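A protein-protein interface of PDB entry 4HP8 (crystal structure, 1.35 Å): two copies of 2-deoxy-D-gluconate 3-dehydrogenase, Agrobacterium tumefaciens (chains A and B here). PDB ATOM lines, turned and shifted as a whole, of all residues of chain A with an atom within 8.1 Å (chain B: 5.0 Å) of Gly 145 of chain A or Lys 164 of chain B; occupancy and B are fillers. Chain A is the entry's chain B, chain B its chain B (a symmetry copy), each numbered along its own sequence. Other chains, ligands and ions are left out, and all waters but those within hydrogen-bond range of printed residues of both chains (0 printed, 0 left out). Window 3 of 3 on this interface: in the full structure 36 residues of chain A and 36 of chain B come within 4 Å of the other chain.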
ATOM      1  N   LEU A 140     -16.182  10.957  -9.999  1.00  0.00           N
ATOM      2  CA  LEU A 140     -14.818  11.294 -10.415  1.00  0.00           C
ATOM      3  C   LEU A 140     -14.635  11.035 -11.913  1.00  0.00           C
ATOM      4  O   LEU A 140     -13.807  11.698 -12.548  1.00  0.00           O
ATOM      5  CB  LEU A 140     -13.768  10.486  -9.612  1.00  0.00           C
ATOM      6  CG  LEU A 140     -13.734  10.807  -8.115  1.00  0.00           C
ATOM      7  CD1 LEU A 140     -12.798   9.790  -7.427  1.00  0.00           C
ATOM      8  CD2 LEU A 140     -13.296  12.223  -7.910  1.00  0.00           C
ATOM      9  N   LEU A 141     -15.376  10.071 -12.447  1.00  0.00           N
ATOM     10  CA  LEU A 141     -15.286   9.730 -13.859  1.00  0.00           C
ATOM     11  C   LEU A 141     -16.134  10.656 -14.741  1.00  0.00           C
ATOM     12  O   LEU A 141     -16.373  10.342 -15.925  1.00  0.00           O
ATOM     13  CB  LEU A 141     -15.616   8.239 -14.059  1.00  0.00           C
ATOM     14  CG  LEU A 141     -14.715   7.313 -13.240  1.00  0.00           C
ATOM     15  CD1 LEU A 141     -14.950   5.877 -13.636  1.00  0.00           C
ATOM     16  CD2 LEU A 141     -13.259   7.660 -13.453  1.00  0.00           C
ATOM     17  N   SER A 142     -16.561  11.801 -14.180  1.00  0.00           N
ATOM     18  CA  SER A 142     -16.941  12.967 -14.985  1.00  0.00           C
ATOM     19  C   SER A 142     -15.733  13.832 -15.318  1.00  0.00           C
ATOM     20  O   SER A 142     -15.847  14.753 -16.147  1.00  0.00           O
ATOM     21  CB  SER A 142     -17.916  13.855 -14.212  1.00  0.00           C
ATOM     22  OG  SER A 142     -19.121  13.181 -13.873  1.00  0.00           O
ATOM     23  N   PHE A 143     -14.604  13.598 -14.647  1.00  0.00           N
ATOM     24  CA  PHE A 143     -13.375  14.409 -14.785  1.00  0.00           C
ATOM     25  C   PHE A 143     -12.182  13.611 -15.292  1.00  0.00           C
ATOM     26  O   PHE A 143     -11.404  14.085 -16.150  1.00  0.00           O
ATOM     27  CB  PHE A 143     -12.930  14.941 -13.415  1.00  0.00           C
ATOM     28  CG  PHE A 143     -13.898  15.912 -12.757  1.00  0.00           C
ATOM     29  CD1 PHE A 143     -14.982  15.461 -12.018  1.00  0.00           C
ATOM     30  CD2 PHE A 143     -13.644  17.275 -12.782  1.00  0.00           C
ATOM     31  CE1 PHE A 143     -15.865  16.381 -11.413  1.00  0.00           C
ATOM     32  CE2 PHE A 143     -14.485  18.203 -12.157  1.00  0.00           C
ATOM     33  CZ  PHE A 143     -15.607  17.754 -11.466  1.00  0.00           C
ATOM     34  N   GLN A 144     -11.983  12.421 -14.734  1.00  0.00           N
ATOM     35  CA  GLN A 144     -10.929  11.504 -15.170  1.00  0.00           C
ATOM     36  C   GLN A 144     -11.541  10.345 -15.939  1.00  0.00           C
ATOM     37  O   GLN A 144     -12.769  10.209 -16.019  1.00  0.00           O
ATOM     38  CB  GLN A 144     -10.113  11.021 -13.953  1.00  0.00           C
ATOM     39  CG  GLN A 144      -9.319  12.215 -13.386  1.00  0.00           C
ATOM     40  CD  GLN A 144      -8.719  11.989 -12.027  1.00  0.00           C
ATOM     41  OE1 GLN A 144      -9.085  11.050 -11.329  1.00  0.00           O
ATOM     42  NE2 GLN A 144      -7.793  12.862 -11.654  1.00  0.00           N
ATOM     43  N   GLY A 145     -10.712   9.460 -16.475  1.00  0.00           N
ATOM     44  CA  GLY A 145     -11.203   8.426 -17.378  1.00  0.00           C
ATOM     45  C   GLY A 145     -11.562   7.102 -16.728  1.00  0.00           C
ATOM     46  O   GLY A 145     -12.480   6.430 -17.184  1.00  0.00           O
ATOM     47  N   GLY A 146     -10.792   6.662 -15.729  1.00  0.00           N
ATOM     48  CA  GLY A 146     -10.944   5.263 -15.267  1.00  0.00           C
ATOM     49  C   GLY A 146     -10.545   4.284 -16.354  1.00  0.00           C
ATOM     50  O   GLY A 146      -9.957   4.678 -17.372  1.00  0.00           O
ATOM     51  N   ILE A 147     -10.775   2.984 -16.137  1.00  0.00           N
ATOM     52  CA  ILE A 147     -10.488   1.983 -17.154  1.00  0.00           C
ATOM     53  C   ILE A 147     -11.638   0.959 -17.128  1.00  0.00           C
ATOM     54  O   ILE A 147     -12.282   0.754 -16.073  1.00  0.00           O
ATOM     55  CB  ILE A 147      -9.117   1.213 -16.949  1.00  0.00           C
ATOM     56  CG1 ILE A 147      -9.090   0.522 -15.571  1.00  0.00           C
ATOM     57  CG2 ILE A 147      -7.892   2.116 -17.222  1.00  0.00           C
ATOM     58  CD1 ILE A 147      -7.894  -0.467 -15.419  1.00  0.00           C
ATOM     59  N   ARG A 148     -11.887   0.314 -18.254  1.00  0.00           N
ATOM     60  CA  ARG A 148     -12.810  -0.851 -18.324  1.00  0.00           C
ATOM     61  C   ARG A 148     -14.262  -0.524 -18.056  1.00  0.00           C
ATOM     62  O   ARG A 148     -15.089  -1.431 -17.968  1.00  0.00           O
ATOM     63  CB  ARG A 148     -12.331  -2.046 -17.469  1.00  0.00           C
ATOM     64  CG  ARG A 148     -10.942  -2.522 -17.888  1.00  0.00           C
ATOM     65  CD  ARG A 148     -10.480  -3.715 -17.036  1.00  0.00           C
ATOM     66  NE  ARG A 148     -11.195  -4.940 -17.379  1.00  0.00           N
ATOM     67  CZ  ARG A 148     -12.019  -5.579 -16.564  1.00  0.00           C
ATOM     68  NH1 ARG A 148     -12.262  -5.107 -15.350  1.00  0.00           N
ATOM     69  NH2 ARG A 148     -12.605  -6.697 -16.967  1.00  0.00           N
ATOM     70  N   VAL A 149     -14.586   0.771 -18.010  1.00  0.00           N
ATOM     71  CA  VAL A 149     -15.970   1.208 -17.782  1.00  0.00           C
ATOM     72  C   VAL A 149     -16.362   2.280 -18.799  1.00  0.00           C
ATOM     73  O   VAL A 149     -16.910   3.338 -18.439  1.00  0.00           O
ATOM     74  CB  VAL A 149     -16.202   1.655 -16.322  1.00  0.00           C
ATOM     75  CG1 VAL A 149     -16.041   0.465 -15.330  1.00  0.00           C
ATOM     76  CG2 VAL A 149     -15.280   2.829 -15.894  1.00  0.00           C
ATOM     77  N   PRO A 150     -16.179   2.020 -20.098  1.00  0.00           N
ATOM     78  CA  PRO A 150     -16.357   3.119 -21.067  1.00  0.00           C
ATOM     79  C   PRO A 150     -17.764   3.721 -21.049  1.00  0.00           C
ATOM     80  O   PRO A 150     -17.899   4.949 -21.130  1.00  0.00           O
ATOM     81  CB  PRO A 150     -16.034   2.456 -22.439  1.00  0.00           C
ATOM     82  CG  PRO A 150     -16.114   0.954 -22.157  1.00  0.00           C
ATOM     83  CD  PRO A 150     -15.621   0.806 -20.749  1.00  0.00           C
ATOM     84  N   TYR A 152     -19.782   3.984 -18.528  1.00  0.00           N
ATOM     85  CA  TYR A 152     -19.971   4.729 -17.296  1.00  0.00           C
ATOM     86  C   TYR A 152     -19.252   6.072 -17.379  1.00  0.00           C
ATOM     87  O   TYR A 152     -19.836   7.101 -17.054  1.00  0.00           O
ATOM     88  CB  TYR A 152     -19.452   3.888 -16.119  1.00  0.00           C
ATOM     89  CG  TYR A 152     -19.671   4.536 -14.770  1.00  0.00           C
ATOM     90  CD1 TYR A 152     -20.869   4.304 -14.096  1.00  0.00           C
ATOM     91  CD2 TYR A 152     -18.703   5.363 -14.174  1.00  0.00           C
ATOM     92  CE1 TYR A 152     -21.117   4.871 -12.834  1.00  0.00           C
ATOM     93  CE2 TYR A 152     -18.951   5.946 -12.901  1.00  0.00           C
ATOM     94  CZ  TYR A 152     -20.151   5.650 -12.251  1.00  0.00           C
ATOM     95  OH  TYR A 152     -20.366   6.249 -11.002  1.00  0.00           O
ATOM     96  N   THR A 153     -17.975   6.089 -17.786  1.00  0.00           N
ATOM     97  CA  THR A 153     -17.225   7.364 -17.937  1.00  0.00           C
ATOM     98  C   THR A 153     -17.885   8.255 -18.943  1.00  0.00           C
ATOM     99  O   THR A 153     -18.063   9.475 -18.705  1.00  0.00           O
ATOM    100  CB  THR A 153     -15.811   7.029 -18.319  1.00  0.00           C
ATOM    101  OG1 THR A 153     -15.251   6.275 -17.217  1.00  0.00           O
ATOM    102  CG2 THR A 153     -15.000   8.280 -18.545  1.00  0.00           C
ATOM    103  N   ALA A 154     -18.319   7.689 -20.082  1.00  0.00           N
ATOM    104  CA  ALA A 154     -19.001   8.522 -21.083  1.00  0.00           C
ATOM    105  C   ALA A 154     -20.296   9.066 -20.513  1.00  0.00           C
ATOM    106  O   ALA A 154     -20.556  10.262 -20.697  1.00  0.00           O
ATOM    107  CB  ALA A 154     -19.261   7.727 -22.363  1.00  0.00           C
ATOM    108  N   HIS A 157     -19.468  11.794 -17.748  1.00  0.00           N
ATOM    109  CA  HIS A 157     -19.093  13.035 -18.447  1.00  0.00           C
ATOM    110  C   HIS A 157     -20.341  13.665 -19.035  1.00  0.00           C
ATOM    111  O   HIS A 157     -20.541  14.897 -18.861  1.00  0.00           O
ATOM    112  CB  HIS A 157     -18.070  12.737 -19.549  1.00  0.00           C
ATOM    113  CG  HIS A 157     -16.637  12.788 -19.098  1.00  0.00           C
ATOM    114  ND1 HIS A 157     -16.087  11.869 -18.227  1.00  0.00           N
ATOM    115  CD2 HIS A 157     -15.644  13.659 -19.432  1.00  0.00           C
ATOM    116  CE1 HIS A 157     -14.804  12.188 -18.052  1.00  0.00           C
ATOM    117  NE2 HIS A 157     -14.517  13.263 -18.763  1.00  0.00           N
ATOM    118  N   ARG A 206      -4.587   7.471  -2.992  1.00  0.00           N
ATOM    119  CA  ARG A 206      -4.945   8.637  -3.798  1.00  0.00           C
ATOM    120  C   ARG A 206      -5.981   9.528  -3.174  1.00  0.00           C
ATOM    121  O   ARG A 206      -6.357  10.534  -3.774  1.00  0.00           O
ATOM    122  CB  ARG A 206      -5.381   8.172  -5.205  1.00  0.00           C
ATOM    123  CG  ARG A 206      -4.174   7.939  -6.138  1.00  0.00           C
ATOM    124  CD  ARG A 206      -4.548   7.711  -7.561  1.00  0.00           C
ATOM    125  NE  ARG A 206      -5.062   8.931  -8.185  1.00  0.00           N
ATOM    126  CZ  ARG A 206      -5.521   8.963  -9.424  1.00  0.00           C
ATOM    127  NH1 ARG A 206      -5.444   7.878 -10.178  1.00  0.00           N
ATOM    128  NH2 ARG A 206      -6.028  10.061  -9.929  1.00  0.00           N
ATOM    129  N   ALA B 160     -14.989  13.383 -24.746  1.00  0.00           N
ATOM    130  CA  ALA B 160     -13.849  13.688 -23.921  1.00  0.00           C
ATOM    131  C   ALA B 160     -13.608  12.588 -22.873  1.00  0.00           C
ATOM    132  O   ALA B 160     -12.462  12.186 -22.630  1.00  0.00           O
ATOM    133  CB  ALA B 160     -14.048  15.035 -23.251  1.00  0.00           C
ATOM    134  N   GLY B 161     -14.676  12.074 -22.257  1.00  0.00           N
ATOM    135  CA  GLY B 161     -14.509  10.993 -21.298  1.00  0.00           C
ATOM    136  C   GLY B 161     -13.911   9.741 -21.922  1.00  0.00           C
ATOM    137  O   GLY B 161     -13.015   9.130 -21.304  1.00  0.00           O
ATOM    138  N   LEU B 162     -14.405   9.320 -23.088  1.00  0.00           N
ATOM    139  CA  LEU B 162     -13.827   8.156 -23.740  1.00  0.00           C
ATOM    140  C   LEU B 162     -12.395   8.402 -24.112  1.00  0.00           C
ATOM    141  O   LEU B 162     -11.590   7.444 -24.080  1.00  0.00           O
ATOM    142  CB  LEU B 162     -14.601   7.785 -25.015  1.00  0.00           C
ATOM    143  CG  LEU B 162     -16.037   7.273 -24.779  1.00  0.00           C
ATOM    144  CD1 LEU B 162     -16.702   7.085 -26.160  1.00  0.00           C
ATOM    145  CD2 LEU B 162     -16.059   5.996 -23.986  1.00  0.00           C
ATOM    146  N   THR B 163     -12.041   9.634 -24.525  1.00  0.00           N
ATOM    147  CA  THR B 163     -10.661   9.904 -24.883  1.00  0.00           C
ATOM    148  C   THR B 163      -9.762   9.599 -23.678  1.00  0.00           C
ATOM    149  O   THR B 163      -8.680   8.998 -23.826  1.00  0.00           O
ATOM    150  CB  THR B 163     -10.551  11.357 -25.311  1.00  0.00           C
ATOM    151  OG1 THR B 163     -11.359  11.560 -26.481  1.00  0.00           O
ATOM    152  CG2 THR B 163      -9.128  11.715 -25.651  1.00  0.00           C
ATOM    153  N   LYS B 164     -10.160  10.056 -22.486  1.00  0.00           N
ATOM    154  CA  LYS B 164      -9.395   9.807 -21.265  1.00  0.00           C
ATOM    155  C   LYS B 164      -9.353   8.334 -20.876  1.00  0.00           C
ATOM    156  O   LYS B 164      -8.269   7.801 -20.596  1.00  0.00           O
ATOM    157  CB  LYS B 164     -10.005  10.621 -20.118  1.00  0.00           C
ATOM    158  CG  LYS B 164      -9.936  12.133 -20.339  1.00  0.00           C
ATOM    159  CD  LYS B 164     -10.854  12.852 -19.330  1.00  0.00           C
ATOM    160  CE  LYS B 164     -11.062  14.284 -19.724  1.00  0.00           C
ATOM    161  NZ  LYS B 164     -12.127  14.857 -18.817  1.00  0.00           N
ATOM    162  N   LEU B 165     -10.504   7.653 -20.885  1.00  0.00           N
ATOM    163  CA  LEU B 165     -10.528   6.253 -20.469  1.00  0.00           C
ATOM    164  C   LEU B 165      -9.726   5.383 -21.422  1.00  0.00           C
ATOM    165  O   LEU B 165      -8.980   4.499 -20.982  1.00  0.00           O
ATOM    166  CB  LEU B 165     -11.983   5.816 -20.384  1.00  0.00           C
ATOM    167  CG  LEU B 165     -12.149   4.304 -20.096  1.00  0.00           C
ATOM    168  CD1 LEU B 165     -13.320   4.012 -19.136  1.00  0.00           C
ATOM    169  CD2 LEU B 165     -12.305   3.486 -21.368  1.00  0.00           C
ATOM    170  N   LEU B 166      -9.882   5.593 -22.723  1.00  0.00           N
ATOM    171  CA  LEU B 166      -9.208   4.725 -23.656  1.00  0.00           C
ATOM    172  C   LEU B 166      -7.695   4.975 -23.626  1.00  0.00           C
ATOM    173  O   LEU B 166      -6.929   4.021 -23.771  1.00  0.00           O
ATOM    174  CB  LEU B 166      -9.798   4.822 -25.056  1.00  0.00           C
ATOM    175  CG  LEU B 166     -11.249   4.374 -25.131  1.00  0.00           C
ATOM    176  CD1 LEU B 166     -11.844   4.755 -26.522  1.00  0.00           C
ATOM    177  CD2 LEU B 166     -11.422   2.875 -24.866  1.00  0.00           C
ATOM    178  N   ALA B 167      -7.274   6.216 -23.424  1.00  0.00           N
ATOM    179  CA  ALA B 167      -5.857   6.480 -23.211  1.00  0.00           C
ATOM    180  C   ALA B 167      -5.373   5.745 -21.934  1.00  0.00           C
ATOM    181  O   ALA B 167      -4.299   5.108 -21.904  1.00  0.00           O
ATOM    182  CB  ALA B 167      -5.623   7.974 -23.080  1.00  0.00           C
ATOM    183  N   ASN B 168      -6.183   5.880 -20.883  1.00  0.00           N
ATOM    184  CA  ASN B 168      -5.838   5.244 -19.640  1.00  0.00           C
ATOM    185  C   ASN B 168      -5.595   3.725 -19.823  1.00  0.00           C
ATOM    186  O   ASN B 168      -4.640   3.198 -19.209  1.00  0.00           O
ATOM    187  CB  ASN B 168      -6.943   5.531 -18.634  1.00  0.00           C
ATOM    188  CG  ASN B 168      -6.510   5.287 -17.206  1.00  0.00           C
ATOM    189  OD1 ASN B 168      -5.333   5.022 -16.909  1.00  0.00           O
ATOM    190  ND2 ASN B 168      -7.464   5.399 -16.300  1.00  0.00           N
ATOM    191  N   GLY B 235      -4.543  11.000 -23.954  1.00  0.00           N
ATOM    192  CA  GLY B 235      -5.720  11.395 -23.175  1.00  0.00           C
ATOM    193  C   GLY B 235      -5.917  12.893 -23.179  1.00  0.00           C
ATOM    194  O   GLY B 235      -6.706  13.359 -22.328  1.00  0.00           O
ATOM    195  N   ILE B 237      -7.099  16.691 -24.508  1.00  0.00           N
ATOM    196  CA  ILE B 237      -8.146  17.355 -25.289  1.00  0.00           C
ATOM    197  C   ILE B 237      -7.578  18.729 -25.663  1.00  0.00           C
ATOM    198  O   ILE B 237      -7.511  19.629 -24.795  1.00  0.00           O
ATOM    199  CB  ILE B 237      -9.439  17.516 -24.499  1.00  0.00           C
ATOM    200  CG1 ILE B 237      -9.870  16.279 -23.665  1.00  0.00           C
ATOM    201  CG2 ILE B 237     -10.529  18.023 -25.466  1.00  0.00           C
ATOM    202  CD1 ILE B 237     -10.225  15.086 -24.442  1.00  0.00           C
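Among the printed residues, merely in contact across the chains: Gly 145 of chain A with Lys 164 of chain B (3.7 Å), Gly 145 of chain A with Leu 165 of chain B (3.2 Å), Gly 146 of chain A with Leu 165 of chain B (3.5 Å), Ile 147 of chain A with Asn 168 of chain B (3.4 Å), Val 149 of chain A with Leu 165 of chain B (3.5 Å), Pro 150 of chain A with Leu 162 of chain B (3.6 Å), Pro 150 of chain A with Leu 165 of chain B (3.6 Å), Thr 153 of chain A with Gly 161 of chain B (3.5 Å), Thr 153 of chain A with Leu 165 of chain B (3.5 Å), Ala 154 of chain A with Leu 162 of chain B (3.99 Å) and His 157 of chain A with Gly 161 of chain B (3.4 Å).
O of Leu 141 of chain A sits at hydrogen-bond distance from ND1 of His 157 of chain A.
O of Ser 142 of chain A is in hydrogen-bond range of NE2 of His 157 of chain A (3.3 Å).
O of Gly 145 of chain A lies within hydrogen-bond range of OG1 of Thr 153 of chain A.
The backbone carbonyl oxygen (O) of Thr 153 of chain A is in hydrogen-bond range of a ring nitrogen (ND1) of His 157 of chain A, 3.1 Å away.
Of the 16 printed residues of chain A, 9 touch a printed residue of chain B.
Hydrophobic or aromatic side chains of chain A that line the printed part of chain B: Ile 147, Val 149, Pro 150, Ala 154 and His 157.
Printed residues of chain B that touch a printed residue of chain A: Gly 161, Leu 162, Lys 164, Leu 165 and Asn 168.
Hydrophobic or aromatic side chains of chain B that line the printed part of chain A: Leu 162 and Leu 165.
Along chain B the printed residues that touch a printed residue of chain A span positions 161 to 168.
O of Phe 143 of chain A is in hydrogen-bond range of NZ of Lys 164 of chain B, 2.9 Å away.
The side-chain amide nitrogen (ND2) of Asn 168 of chain B sits at hydrogen-bond distance from the backbone carbonyl oxygen (O) of Gly 146 of chain A (2.8 Å).
NE2 of His 157 of chain A is in hydrogen-bond range of NZ of Lys 164 of chain B (2.9 Å).
No position is printed for both chains.
Of the 14 pairs that touch across the chains among the printed residues, none has its exchanged pair printed and touching as well.
Of the printed residues of chain B, Gly 145 of chain A touches Lys 164 (3.7 Å) and Leu 165 (3.2 Å).
Of the printed residues of chain B, Gly 146 of chain A touches Leu 165 (3.5 Å) and Asn 168 (2.8 Å).
Printed residues of chain A within 4 Å of Leu 165 of chain B: Gly 145, Gly 146, Val 149, Pro 150 and Thr 153.
Printed residues of chain B within 4 Å of Thr 153 of chain A: Gly 161 and Leu 165.
Of the printed residues of chain A, Leu 162 of chain B touches Pro 150 and Ala 154.
Printed residues of chain B within 4 Å of Phe 143 of chain A: Lys 164 (2.9 Å).
Arg 206 of chain A touches none of the printed residues of chain B.
The nearest printed residue of chain B that does not touch Gly 145 of chain A is Gly 161 of chain B (4.4 Å).
The nearest printed residue of chain B that does not touch Ile 147 of chain A is Leu 165 of chain B (4.01 Å).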
